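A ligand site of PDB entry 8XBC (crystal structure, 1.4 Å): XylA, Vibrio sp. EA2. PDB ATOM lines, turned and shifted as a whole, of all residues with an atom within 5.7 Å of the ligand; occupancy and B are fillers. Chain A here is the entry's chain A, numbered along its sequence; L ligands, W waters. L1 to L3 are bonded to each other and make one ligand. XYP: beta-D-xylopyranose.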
ATOM      1  N   ILE A  35      23.570  -3.047  -1.775  1.00  0.00           N
ATOM      2  CA  ILE A  35      23.105  -4.419  -1.716  1.00  0.00           C
ATOM      3  C   ILE A  35      21.586  -4.542  -1.920  1.00  0.00           C
ATOM      4  O   ILE A  35      21.018  -5.614  -1.683  1.00  0.00           O
ATOM      5  CB  ILE A  35      23.515  -5.096  -0.391  1.00  0.00           C
ATOM      6  CG1 ILE A  35      22.803  -4.441   0.795  1.00  0.00           C
ATOM      7  CG2 ILE A  35      25.041  -5.030  -0.202  1.00  0.00           C
ATOM      8  CD1 ILE A  35      22.829  -5.285   2.051  1.00  0.00           C
ATOM      9  N   GLU A  36      20.906  -3.457  -2.307  1.00  0.00           N
ATOM     10  CA  GLU A  36      19.451  -3.502  -2.405  1.00  0.00           C
ATOM     11  C   GLU A  36      18.985  -4.284  -3.624  1.00  0.00           C
ATOM     12  O   GLU A  36      19.514  -4.120  -4.732  1.00  0.00           O
ATOM     13  CB  GLU A  36      18.855  -2.097  -2.438  1.00  0.00           C
ATOM     14  CG  GLU A  36      19.230  -1.209  -1.279  1.00  0.00           C
ATOM     15  CD  GLU A  36      18.910  -1.808   0.083  1.00  0.00           C
ATOM     16  OE1 GLU A  36      19.815  -1.788   0.945  1.00  0.00           O
ATOM     17  OE2 GLU A  36      17.740  -2.234   0.314  1.00  0.00           O
ATOM     18  N   THR A  37      17.958  -5.115  -3.436  1.00  0.00           N
ATOM     19  CA  THR A  37      17.317  -5.848  -4.509  1.00  0.00           C
ATOM     20  C   THR A  37      15.861  -5.471  -4.749  1.00  0.00           C
ATOM     21  O   THR A  37      15.313  -5.817  -5.804  1.00  0.00           O
ATOM     22  CB  THR A  37      17.337  -7.358  -4.217  1.00  0.00           C
ATOM     23  OG1 THR A  37      16.595  -7.605  -3.011  1.00  0.00           O
ATOM     24  CG2 THR A  37      18.769  -7.868  -4.054  1.00  0.00           C
ATOM     25  N   ASP A  38      15.218  -4.800  -3.817  1.00  0.00           N
ATOM     26  CA  ASP A  38      13.781  -4.573  -3.927  1.00  0.00           C
ATOM     27  C   ASP A  38      13.488  -3.651  -5.105  1.00  0.00           C
ATOM     28  O   ASP A  38      14.072  -2.572  -5.208  1.00  0.00           O
ATOM     29  CB  ASP A  38      13.246  -3.972  -2.635  1.00  0.00           C
ATOM     30  CG  ASP A  38      11.737  -3.838  -2.651  1.00  0.00           C
ATOM     31  OD1 ASP A  38      11.242  -2.863  -3.251  1.00  0.00           O
ATOM     32  OD2 ASP A  38      11.044  -4.703  -2.075  1.00  0.00           O
ATOM     33  N   GLU A  67      25.337  -8.309  -4.436  1.00  0.00           N
ATOM     34  CA  GLU A  67      24.521  -9.030  -3.476  1.00  0.00           C
ATOM     35  C   GLU A  67      25.217  -9.076  -2.118  1.00  0.00           C
ATOM     36  O   GLU A  67      26.439  -9.221  -2.034  1.00  0.00           O
ATOM     37  CB  GLU A  67      24.253 -10.441  -3.995  1.00  0.00           C
ATOM     38  CG  GLU A  67      23.403 -11.314  -3.104  1.00  0.00           C
ATOM     39  CD  GLU A  67      24.228 -12.042  -2.049  1.00  0.00           C
ATOM     40  OE1 GLU A  67      25.410 -12.326  -2.327  1.00  0.00           O
ATOM     41  OE2 GLU A  67      23.683 -12.287  -0.942  1.00  0.00           O
ATOM     42  N   ASN A  68      24.404  -9.024  -1.052  1.00  0.00           N
ATOM     43  CA  ASN A  68      24.856  -8.950   0.331  1.00  0.00           C
ATOM     44  C   ASN A  68      26.082  -9.807   0.629  1.00  0.00           C
ATOM     45  O   ASN A  68      27.139  -9.298   1.020  1.00  0.00           O
ATOM     46  CB  ASN A  68      23.664  -9.352   1.219  1.00  0.00           C
ATOM     47  CG  ASN A  68      23.961  -9.309   2.702  1.00  0.00           C
ATOM     48  OD1 ASN A  68      24.539  -8.365   3.222  1.00  0.00           O
ATOM     49  ND2 ASN A  68      23.496 -10.332   3.400  1.00  0.00           N
ATOM     50  N   GLU A  69      25.967 -11.128   0.449  1.00  0.00           N
ATOM     51  CA  GLU A  69      27.078 -12.014   0.772  1.00  0.00           C
ATOM     52  C   GLU A  69      28.310 -11.712  -0.091  1.00  0.00           C
ATOM     53  O   GLU A  69      29.435 -11.629   0.408  1.00  0.00           O
ATOM     54  CB  GLU A  69      26.630 -13.473   0.612  1.00  0.00           C
ATOM     55  CG  GLU A  69      25.705 -13.956   1.735  1.00  0.00           C
ATOM     56  CD  GLU A  69      26.251 -13.682   3.127  1.00  0.00           C
ATOM     57  OE1 GLU A  69      25.578 -13.022   3.933  1.00  0.00           O
ATOM     58  OE2 GLU A  69      27.380 -14.136   3.413  1.00  0.00           O
ATOM     59  N   LYS A  72      29.988  -8.328   1.091  1.00  0.00           N
ATOM     60  CA  LYS A  72      30.827  -8.447   2.277  1.00  0.00           C
ATOM     61  C   LYS A  72      32.150  -9.160   1.973  1.00  0.00           C
ATOM     62  O   LYS A  72      33.198  -8.768   2.503  1.00  0.00           O
ATOM     63  CB  LYS A  72      30.065  -9.172   3.395  1.00  0.00           C
ATOM     64  CG  LYS A  72      28.891  -8.365   3.946  1.00  0.00           C
ATOM     65  CD  LYS A  72      28.204  -9.116   5.080  1.00  0.00           C
ATOM     66  CE  LYS A  72      27.551 -10.382   4.561  1.00  0.00           C
ATOM     67  NZ  LYS A  72      26.667 -11.053   5.549  1.00  0.00           N
ATOM     68  N   TYR A  89      27.889   0.677   0.931  1.00  0.00           N
ATOM     69  CA  TYR A  89      27.024   0.344   2.055  1.00  0.00           C
ATOM     70  C   TYR A  89      27.846  -0.114   3.246  1.00  0.00           C
ATOM     71  O   TYR A  89      28.834  -0.837   3.086  1.00  0.00           O
ATOM     72  CB  TYR A  89      26.084  -0.785   1.658  1.00  0.00           C
ATOM     73  CG  TYR A  89      24.899  -1.050   2.571  1.00  0.00           C
ATOM     74  CD1 TYR A  89      23.863  -0.137   2.653  1.00  0.00           C
ATOM     75  CD2 TYR A  89      24.794  -2.221   3.296  1.00  0.00           C
ATOM     76  CE1 TYR A  89      22.737  -0.388   3.442  1.00  0.00           C
ATOM     77  CE2 TYR A  89      23.676  -2.479   4.105  1.00  0.00           C
ATOM     78  CZ  TYR A  89      22.656  -1.558   4.159  1.00  0.00           C
ATOM     79  OH  TYR A  89      21.524  -1.826   4.925  1.00  0.00           O
ATOM     80  N   TRP A  91      27.599  -1.224   7.671  1.00  0.00           N
ATOM     81  CA  TRP A  91      26.894  -1.481   8.911  1.00  0.00           C
ATOM     82  C   TRP A  91      27.509  -0.741  10.093  1.00  0.00           C
ATOM     83  O   TRP A  91      27.135  -0.993  11.240  1.00  0.00           O
ATOM     84  CB  TRP A  91      26.881  -2.988   9.210  1.00  0.00           C
ATOM     85  CG  TRP A  91      26.045  -3.791   8.240  1.00  0.00           C
ATOM     86  CD1 TRP A  91      24.747  -4.169   8.400  1.00  0.00           C
ATOM     87  CD2 TRP A  91      26.450  -4.312   6.962  1.00  0.00           C
ATOM     88  NE1 TRP A  91      24.318  -4.900   7.321  1.00  0.00           N
ATOM     89  CE2 TRP A  91      25.347  -4.987   6.418  1.00  0.00           C
ATOM     90  CE3 TRP A  91      27.658  -4.275   6.242  1.00  0.00           C
ATOM     91  CZ2 TRP A  91      25.404  -5.629   5.170  1.00  0.00           C
ATOM     92  CZ3 TRP A  91      27.712  -4.897   5.016  1.00  0.00           C
ATOM     93  CH2 TRP A  91      26.588  -5.566   4.491  1.00  0.00           C
ATOM     94  N   MET A 139      19.576   4.166   7.505  1.00  0.00           N
ATOM     95  CA  MET A 139      18.416   3.564   8.145  1.00  0.00           C
ATOM     96  C   MET A 139      18.717   2.988   9.509  1.00  0.00           C
ATOM     97  O   MET A 139      19.851   2.737   9.835  1.00  0.00           O
ATOM     98  CB  MET A 139      17.798   2.459   7.252  1.00  0.00           C
ATOM     99  CG  MET A 139      18.700   1.276   6.937  1.00  0.00           C
ATOM    100  SD  MET A 139      18.633   0.005   8.212  1.00  0.00           S
ATOM    101  CE  MET A 139      18.548  -1.504   7.259  1.00  0.00           C
ATOM    102  N   SER A 141      17.203  -0.263  12.089  1.00  0.00           N
ATOM    103  CA  SER A 141      16.418  -1.470  11.955  1.00  0.00           C
ATOM    104  C   SER A 141      16.254  -2.242  13.247  1.00  0.00           C
ATOM    105  O   SER A 141      17.001  -2.005  14.193  1.00  0.00           O
ATOM    106  CB  SER A 141      17.059  -2.422  10.894  1.00  0.00           C
ATOM    107  OG  SER A 141      18.306  -2.909  11.332  1.00  0.00           O
ATOM    108  N   TRP A 191      24.505 -15.841   9.415  1.00  0.00           N
ATOM    109  CA  TRP A 191      24.001 -14.694  10.155  1.00  0.00           C
ATOM    110  C   TRP A 191      22.504 -14.757  10.536  1.00  0.00           C
ATOM    111  O   TRP A 191      22.163 -14.321  11.581  1.00  0.00           O
ATOM    112  CB  TRP A 191      24.430 -13.363   9.513  1.00  0.00           C
ATOM    113  CG  TRP A 191      23.803 -13.080   8.145  1.00  0.00           C
ATOM    114  CD1 TRP A 191      24.362 -13.314   6.922  1.00  0.00           C
ATOM    115  CD2 TRP A 191      22.507 -12.507   7.882  1.00  0.00           C
ATOM    116  NE1 TRP A 191      23.498 -12.942   5.920  1.00  0.00           N
ATOM    117  CE2 TRP A 191      22.351 -12.450   6.485  1.00  0.00           C
ATOM    118  CE3 TRP A 191      21.465 -12.066   8.686  1.00  0.00           C
ATOM    119  CZ2 TRP A 191      21.199 -11.949   5.887  1.00  0.00           C
ATOM    120  CZ3 TRP A 191      20.326 -11.583   8.088  1.00  0.00           C
ATOM    121  CH2 TRP A 191      20.204 -11.521   6.705  1.00  0.00           C
ATOM    122  N   HIS A 194      22.670 -16.581  13.685  1.00  0.00           N
ATOM    123  CA  HIS A 194      23.312 -15.823  14.741  1.00  0.00           C
ATOM    124  C   HIS A 194      22.405 -14.869  15.488  1.00  0.00           C
ATOM    125  O   HIS A 194      22.655 -14.559  16.597  1.00  0.00           O
ATOM    126  CB  HIS A 194      24.634 -15.230  14.259  1.00  0.00           C
ATOM    127  CG  HIS A 194      24.669 -13.747  14.123  1.00  0.00           C
ATOM    128  ND1 HIS A 194      23.962 -13.085  13.146  1.00  0.00           N
ATOM    129  CD2 HIS A 194      25.387 -12.819  14.768  1.00  0.00           C
ATOM    130  CE1 HIS A 194      24.224 -11.795  13.229  1.00  0.00           C
ATOM    131  NE2 HIS A 194      25.090 -11.607  14.204  1.00  0.00           N
ATOM    132  N   PHE A 195      21.309 -14.489  14.855  1.00  0.00           N
ATOM    133  CA  PHE A 195      20.315 -13.660  15.520  1.00  0.00           C
ATOM    134  C   PHE A 195      19.754 -14.358  16.805  1.00  0.00           C
ATOM    135  O   PHE A 195      19.477 -13.705  17.766  1.00  0.00           O
ATOM    136  CB  PHE A 195      19.169 -13.340  14.552  1.00  0.00           C
ATOM    137  CG  PHE A 195      19.493 -12.341  13.471  1.00  0.00           C
ATOM    138  CD1 PHE A 195      20.605 -11.529  13.523  1.00  0.00           C
ATOM    139  CD2 PHE A 195      18.627 -12.191  12.397  1.00  0.00           C
ATOM    140  CE1 PHE A 195      20.851 -10.615  12.517  1.00  0.00           C
ATOM    141  CE2 PHE A 195      18.863 -11.274  11.400  1.00  0.00           C
ATOM    142  CZ  PHE A 195      19.978 -10.478  11.471  1.00  0.00           C
ATOM    143  N   TYR A 251      19.328 -16.631   2.880  1.00  0.00           N
ATOM    144  CA  TYR A 251      18.261 -15.733   3.311  1.00  0.00           C
ATOM    145  C   TYR A 251      17.115 -15.652   2.300  1.00  0.00           C
ATOM    146  O   TYR A 251      15.984 -15.671   2.666  1.00  0.00           O
ATOM    147  CB  TYR A 251      18.893 -14.328   3.639  1.00  0.00           C
ATOM    148  CG  TYR A 251      17.871 -13.257   3.960  1.00  0.00           C
ATOM    149  CD1 TYR A 251      16.755 -13.535   4.747  1.00  0.00           C
ATOM    150  CD2 TYR A 251      18.007 -11.961   3.493  1.00  0.00           C
ATOM    151  CE1 TYR A 251      15.811 -12.591   5.004  1.00  0.00           C
ATOM    152  CE2 TYR A 251      17.073 -10.991   3.774  1.00  0.00           C
ATOM    153  CZ  TYR A 251      15.975 -11.328   4.528  1.00  0.00           C
ATOM    154  OH  TYR A 251      15.023 -10.395   4.813  1.00  0.00           O
ATOM    155  N   TRP A 271      13.388  -5.193   7.241  1.00  0.00           N
ATOM    156  CA  TRP A 271      13.457  -5.209   5.782  1.00  0.00           C
ATOM    157  C   TRP A 271      12.790  -6.468   5.181  1.00  0.00           C
ATOM    158  O   TRP A 271      12.543  -6.547   4.013  1.00  0.00           O
ATOM    159  CB  TRP A 271      14.957  -5.166   5.379  1.00  0.00           C
ATOM    160  CG  TRP A 271      15.796  -6.267   5.904  1.00  0.00           C
ATOM    161  CD1 TRP A 271      15.912  -7.523   5.392  1.00  0.00           C
ATOM    162  CD2 TRP A 271      16.675  -6.218   7.029  1.00  0.00           C
ATOM    163  NE1 TRP A 271      16.786  -8.263   6.147  1.00  0.00           N
ATOM    164  CE2 TRP A 271      17.267  -7.478   7.146  1.00  0.00           C
ATOM    165  CE3 TRP A 271      17.013  -5.209   7.942  1.00  0.00           C
ATOM    166  CZ2 TRP A 271      18.190  -7.775   8.142  1.00  0.00           C
ATOM    167  CZ3 TRP A 271      17.924  -5.511   8.926  1.00  0.00           C
ATOM    168  CH2 TRP A 271      18.506  -6.773   9.022  1.00  0.00           C
ATOM    169  N   PHE A 275      10.725  -8.037   1.602  1.00  0.00           N
ATOM    170  CA  PHE A 275      11.485  -9.120   0.978  1.00  0.00           C
ATOM    171  C   PHE A 275      10.743 -10.447   0.847  1.00  0.00           C
ATOM    172  O   PHE A 275      10.818 -11.066  -0.164  1.00  0.00           O
ATOM    173  CB  PHE A 275      12.854  -9.290   1.672  1.00  0.00           C
ATOM    174  CG  PHE A 275      13.826 -10.153   0.930  1.00  0.00           C
ATOM    175  CD1 PHE A 275      14.157  -9.922  -0.385  1.00  0.00           C
ATOM    176  CD2 PHE A 275      14.426 -11.206   1.574  1.00  0.00           C
ATOM    177  CE1 PHE A 275      15.076 -10.719  -1.035  1.00  0.00           C
ATOM    178  CE2 PHE A 275      15.339 -12.012   0.933  1.00  0.00           C
ATOM    179  CZ  PHE A 275      15.682 -11.755  -0.369  1.00  0.00           C
ATOM    180  N   ASN A 314      22.520   1.456   9.751  1.00  0.00           N
ATOM    181  CA  ASN A 314      23.259   1.205   8.536  1.00  0.00           C
ATOM    182  C   ASN A 314      23.394   2.504   7.757  1.00  0.00           C
ATOM    183  O   ASN A 314      22.610   3.398   7.926  1.00  0.00           O
ATOM    184  CB  ASN A 314      22.606   0.101   7.669  1.00  0.00           C
ATOM    185  CG  ASN A 314      22.588  -1.246   8.336  1.00  0.00           C
ATOM    186  OD1 ASN A 314      22.979  -1.406   9.467  1.00  0.00           O
ATOM    187  ND2 ASN A 314      22.083  -2.229   7.619  1.00  0.00           N
ATOM    188  N   GLN A 347       9.948   0.242   3.544  1.00  0.00           N
ATOM    189  CA  GLN A 347      11.266  -0.368   3.543  1.00  0.00           C
ATOM    190  C   GLN A 347      12.074  -0.057   4.766  1.00  0.00           C
ATOM    191  O   GLN A 347      12.459  -0.944   5.493  1.00  0.00           O
ATOM    192  CB  GLN A 347      12.072   0.055   2.300  1.00  0.00           C
ATOM    193  CG  GLN A 347      13.404  -0.636   2.192  1.00  0.00           C
ATOM    194  CD  GLN A 347      13.278  -2.101   1.814  1.00  0.00           C
ATOM    195  OE1 GLN A 347      12.228  -2.570   1.438  1.00  0.00           O
ATOM    196  NE2 GLN A 347      14.373  -2.821   1.899  1.00  0.00           N
ATOM    197  N   PHE A 380      24.001  -5.667  15.350  1.00  0.00           N
ATOM    198  CA  PHE A 380      24.217  -7.062  15.008  1.00  0.00           C
ATOM    199  C   PHE A 380      25.583  -7.530  15.471  1.00  0.00           C
ATOM    200  O   PHE A 380      26.564  -6.906  15.166  1.00  0.00           O
ATOM    201  CB  PHE A 380      24.151  -7.258  13.465  1.00  0.00           C
ATOM    202  CG  PHE A 380      23.007  -6.539  12.788  1.00  0.00           C
ATOM    203  CD1 PHE A 380      21.714  -6.981  12.913  1.00  0.00           C
ATOM    204  CD2 PHE A 380      23.264  -5.458  11.971  1.00  0.00           C
ATOM    205  CE1 PHE A 380      20.682  -6.328  12.263  1.00  0.00           C
ATOM    206  CE2 PHE A 380      22.241  -4.809  11.321  1.00  0.00           C
ATOM    207  CZ  PHE A 380      20.945  -5.253  11.466  1.00  0.00           C
ATOM    208  N   ASP A 382      27.627  -9.893  14.585  1.00  0.00           N
ATOM    209  CA  ASP A 382      28.625 -10.112  13.544  1.00  0.00           C
ATOM    210  C   ASP A 382      29.238  -8.819  13.040  1.00  0.00           C
ATOM    211  O   ASP A 382      30.387  -8.775  12.750  1.00  0.00           O
ATOM    212  CB  ASP A 382      28.153 -11.099  12.456  1.00  0.00           C
ATOM    213  CG  ASP A 382      27.134 -10.530  11.506  1.00  0.00           C
ATOM    214  OD1 ASP A 382      26.399  -9.620  11.864  1.00  0.00           O
ATOM    215  OD2 ASP A 382      27.081 -11.038  10.369  1.00  0.00           O
ATOM    216  N   GLN A 383      28.435  -7.789  12.947  1.00  0.00           N
ATOM    217  CA  GLN A 383      28.904  -6.485  12.519  1.00  0.00           C
ATOM    218  C   GLN A 383      29.620  -5.704  13.635  1.00  0.00           C
ATOM    219  O   GLN A 383      30.582  -5.038  13.414  1.00  0.00           O
ATOM    220  CB  GLN A 383      27.725  -5.692  11.906  1.00  0.00           C
ATOM    221  CG  GLN A 383      27.118  -6.352  10.682  1.00  0.00           C
ATOM    222  CD  GLN A 383      28.107  -6.463   9.540  1.00  0.00           C
ATOM    223  OE1 GLN A 383      29.011  -5.672   9.405  1.00  0.00           O
ATOM    224  NE2 GLN A 383      27.890  -7.438   8.694  1.00  0.00           N
ATOM    225  N   ASN A 394      29.072 -16.244  13.824  1.00  0.00           N
ATOM    226  CA  ASN A 394      28.221 -16.831  12.792  1.00  0.00           C
ATOM    227  C   ASN A 394      28.467 -18.340  12.675  1.00  0.00           C
ATOM    228  O   ASN A 394      27.530 -19.104  12.657  1.00  0.00           O
ATOM    229  CB  ASN A 394      28.448 -16.122  11.430  1.00  0.00           C
ATOM    230  CG  ASN A 394      27.750 -14.781  11.318  1.00  0.00           C
ATOM    231  OD1 ASN A 394      26.864 -14.483  12.076  1.00  0.00           O
ATOM    232  ND2 ASN A 394      28.170 -13.980  10.381  1.00  0.00           N
HETATM  233  O1  XYP L   1      19.368  -9.867  -1.004  1.00  0.00           O
HETATM  234  C1  XYP L   1      18.559  -9.322   0.028  1.00  0.00           C
HETATM  235  C2  XYP L   1      19.434  -8.488   0.966  1.00  0.00           C
HETATM  236  C3  XYP L   1      18.580  -7.693   1.946  1.00  0.00           C
HETATM  237  C4  XYP L   1      17.484  -6.930   1.208  1.00  0.00           C
HETATM  238  C5  XYP L   1      16.721  -7.916   0.340  1.00  0.00           C
HETATM  239  O2  XYP L   1      20.285  -9.370   1.705  1.00  0.00           O
HETATM  240  O3  XYP L   1      19.451  -6.763   2.478  1.00  0.00           O
HETATM  241  O4  XYP L   1      16.566  -6.305   2.115  1.00  0.00           O
HETATM  242  O5  XYP L   1      17.594  -8.502  -0.608  1.00  0.00           O
HETATM  243  C1  XYP L   2      19.523  -6.595   3.897  1.00  0.00           C
HETATM  244  C2  XYP L   2      20.788  -7.269   4.410  1.00  0.00           C
HETATM  245  C3  XYP L   2      21.120  -6.879   5.840  1.00  0.00           C
HETATM  246  C4  XYP L   2      21.047  -5.370   6.017  1.00  0.00           C
HETATM  247  C5  XYP L   2      19.697  -4.872   5.528  1.00  0.00           C
HETATM  248  O2  XYP L   2      20.570  -8.695   4.360  1.00  0.00           O
HETATM  249  O3  XYP L   2      22.471  -7.266   6.097  1.00  0.00           O
HETATM  250  O4  XYP L   2      21.210  -5.016   7.394  1.00  0.00           O
HETATM  251  O5  XYP L   2      19.615  -5.195   4.143  1.00  0.00           O
HETATM  252  C1  XYP L   3      22.711  -8.161   7.109  1.00  0.00           C
HETATM  253  C2  XYP L   3      24.184  -8.507   7.162  1.00  0.00           C
HETATM  254  C3  XYP L   3      24.453  -9.408   8.349  1.00  0.00           C
HETATM  255  C4  XYP L   3      23.903  -8.752   9.613  1.00  0.00           C
HETATM  256  C5  XYP L   3      22.430  -8.421   9.438  1.00  0.00           C
HETATM  257  O2  XYP L   3      24.507  -9.213   5.968  1.00  0.00           O
HETATM  258  O3  XYP L   3      25.873  -9.580   8.442  1.00  0.00           O
HETATM  259  O4  XYP L   3      24.019  -9.659  10.722  1.00  0.00           O
HETATM  260  O5  XYP L   3      22.284  -7.532   8.325  1.00  0.00           O
HETATM  261  O   HOH W   1      21.226 -11.773   0.640  1.00  0.00           O
HETATM  262  O   HOH W   2      21.697  -8.293  -1.641  1.00  0.00           O
HETATM  263  O   HOH W   3      18.350 -11.595  -2.812  1.00  0.00           O
HETATM  264  O   HOH W   4      17.606  -3.923   2.593  1.00  0.00           O
HETATM  265  O   HOH W   5      14.386  -5.437   0.598  1.00  0.00           O
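The side-chain amide nitrogen (NE2) of Gln 383 sits at hydrogen-bond distance from an oxygen (O3) of XYP L3, 3.0 Å away. The side-chain amino group (NZ) of Lys 72 sits at hydrogen-bond distance from an oxygen (O2) of XYP L3. O2 of XYP L3 sits at hydrogen-bond distance from OD1 of Asn 68 (2.9 Å). O5 of XYP L1 is in hydrogen-bond range of OG1 of Thr 37 (2.8 Å). ND2 of Asn 314 is in hydrogen-bond range of O4 of XYP L2. An oxygen (O4) of XYP L3 is in hydrogen-bond range of the side-chain carboxylate of Asp 382, 2.6 Å away. The indole nitrogen (NE1) of Trp 91 is in hydrogen-bond range of an oxygen (O4) of XYP L2 (3.1 Å).
The side-chain hydroxyl (OH) of Tyr 89 sits at hydrogen-bond distance from the side-chain amide nitrogen (ND2) of Asn 314 (2.8 Å). The side-chain carboxylate of Glu 69 lies within salt-bridge range of the side-chain amino group of Lys 72 (2.8 Å). The indole nitrogen (NE1) of Trp 191 is in hydrogen-bond range of the side-chain carboxylate (OE1) of Glu 69 (2.9 Å). ND2 of Asn 68 is in hydrogen-bond range of OE1 of Glu 69. The backbone NH (N) of Asn 314 lies within hydrogen-bond range of the backbone carbonyl oxygen (O) of Met 139 (3.0 Å). The indole nitrogen (NE1) of Trp 271 lies close to the side-chain hydroxyl (OH) of Tyr 251. N of Asp 382 lies within hydrogen-bond range of NE2 of His 194 (3.1 Å). The side-chain amide oxygen of Asn 394 sits close to a ring nitrogen (ND1) of His 194, 3.4 Å away.
Residues that only touch the ligand: His 194, Phe 275, Trp 271, Tyr 89, Phe 380, Trp 191, Ile 35, Phe 195, Tyr 251 and Met 139. Hydrophobic or aromatic side chains that line the ligand: Ile 35, Trp 91, Met 139, Trp 191, His 194, Phe 195, Tyr 251, Trp 271, Phe 275 and Phe 380. 17 residues have an atom within 4 Å of the ligand: Ile 35, Thr 37, Asn 68, Lys 72, Tyr 89, Trp 91, Met 139, Trp 191, His 194, Phe 195, Tyr 251, Trp 271, Phe 275, Asn 314, Phe 380, Asp 382 and Gln 383. The nearest printed residue that does not touch the ligand is Gln 347 (4.1 Å).
Water W4 lies within hydrogen-bond range of an oxygen (O4) of XYP L1 (2.6 Å), the side-chain carboxylate of Glu 36 (2.8 Å) and the side-chain amide nitrogen of Gln 347 (3.5 Å). Water W1 bridges an oxygen (O2) of XYP L1 and the side-chain carboxylate (OE2) of Glu 67. Water W5 bridges O4 of XYP L1 (2.8 Å) and NE2 of Gln 347 (2.9 Å). Water W2 lies within hydrogen-bond range of O of Ile 35 (2.8 Å), N of Asn 68 (2.9 Å) and O1 of XYP L1 (2.9 Å).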
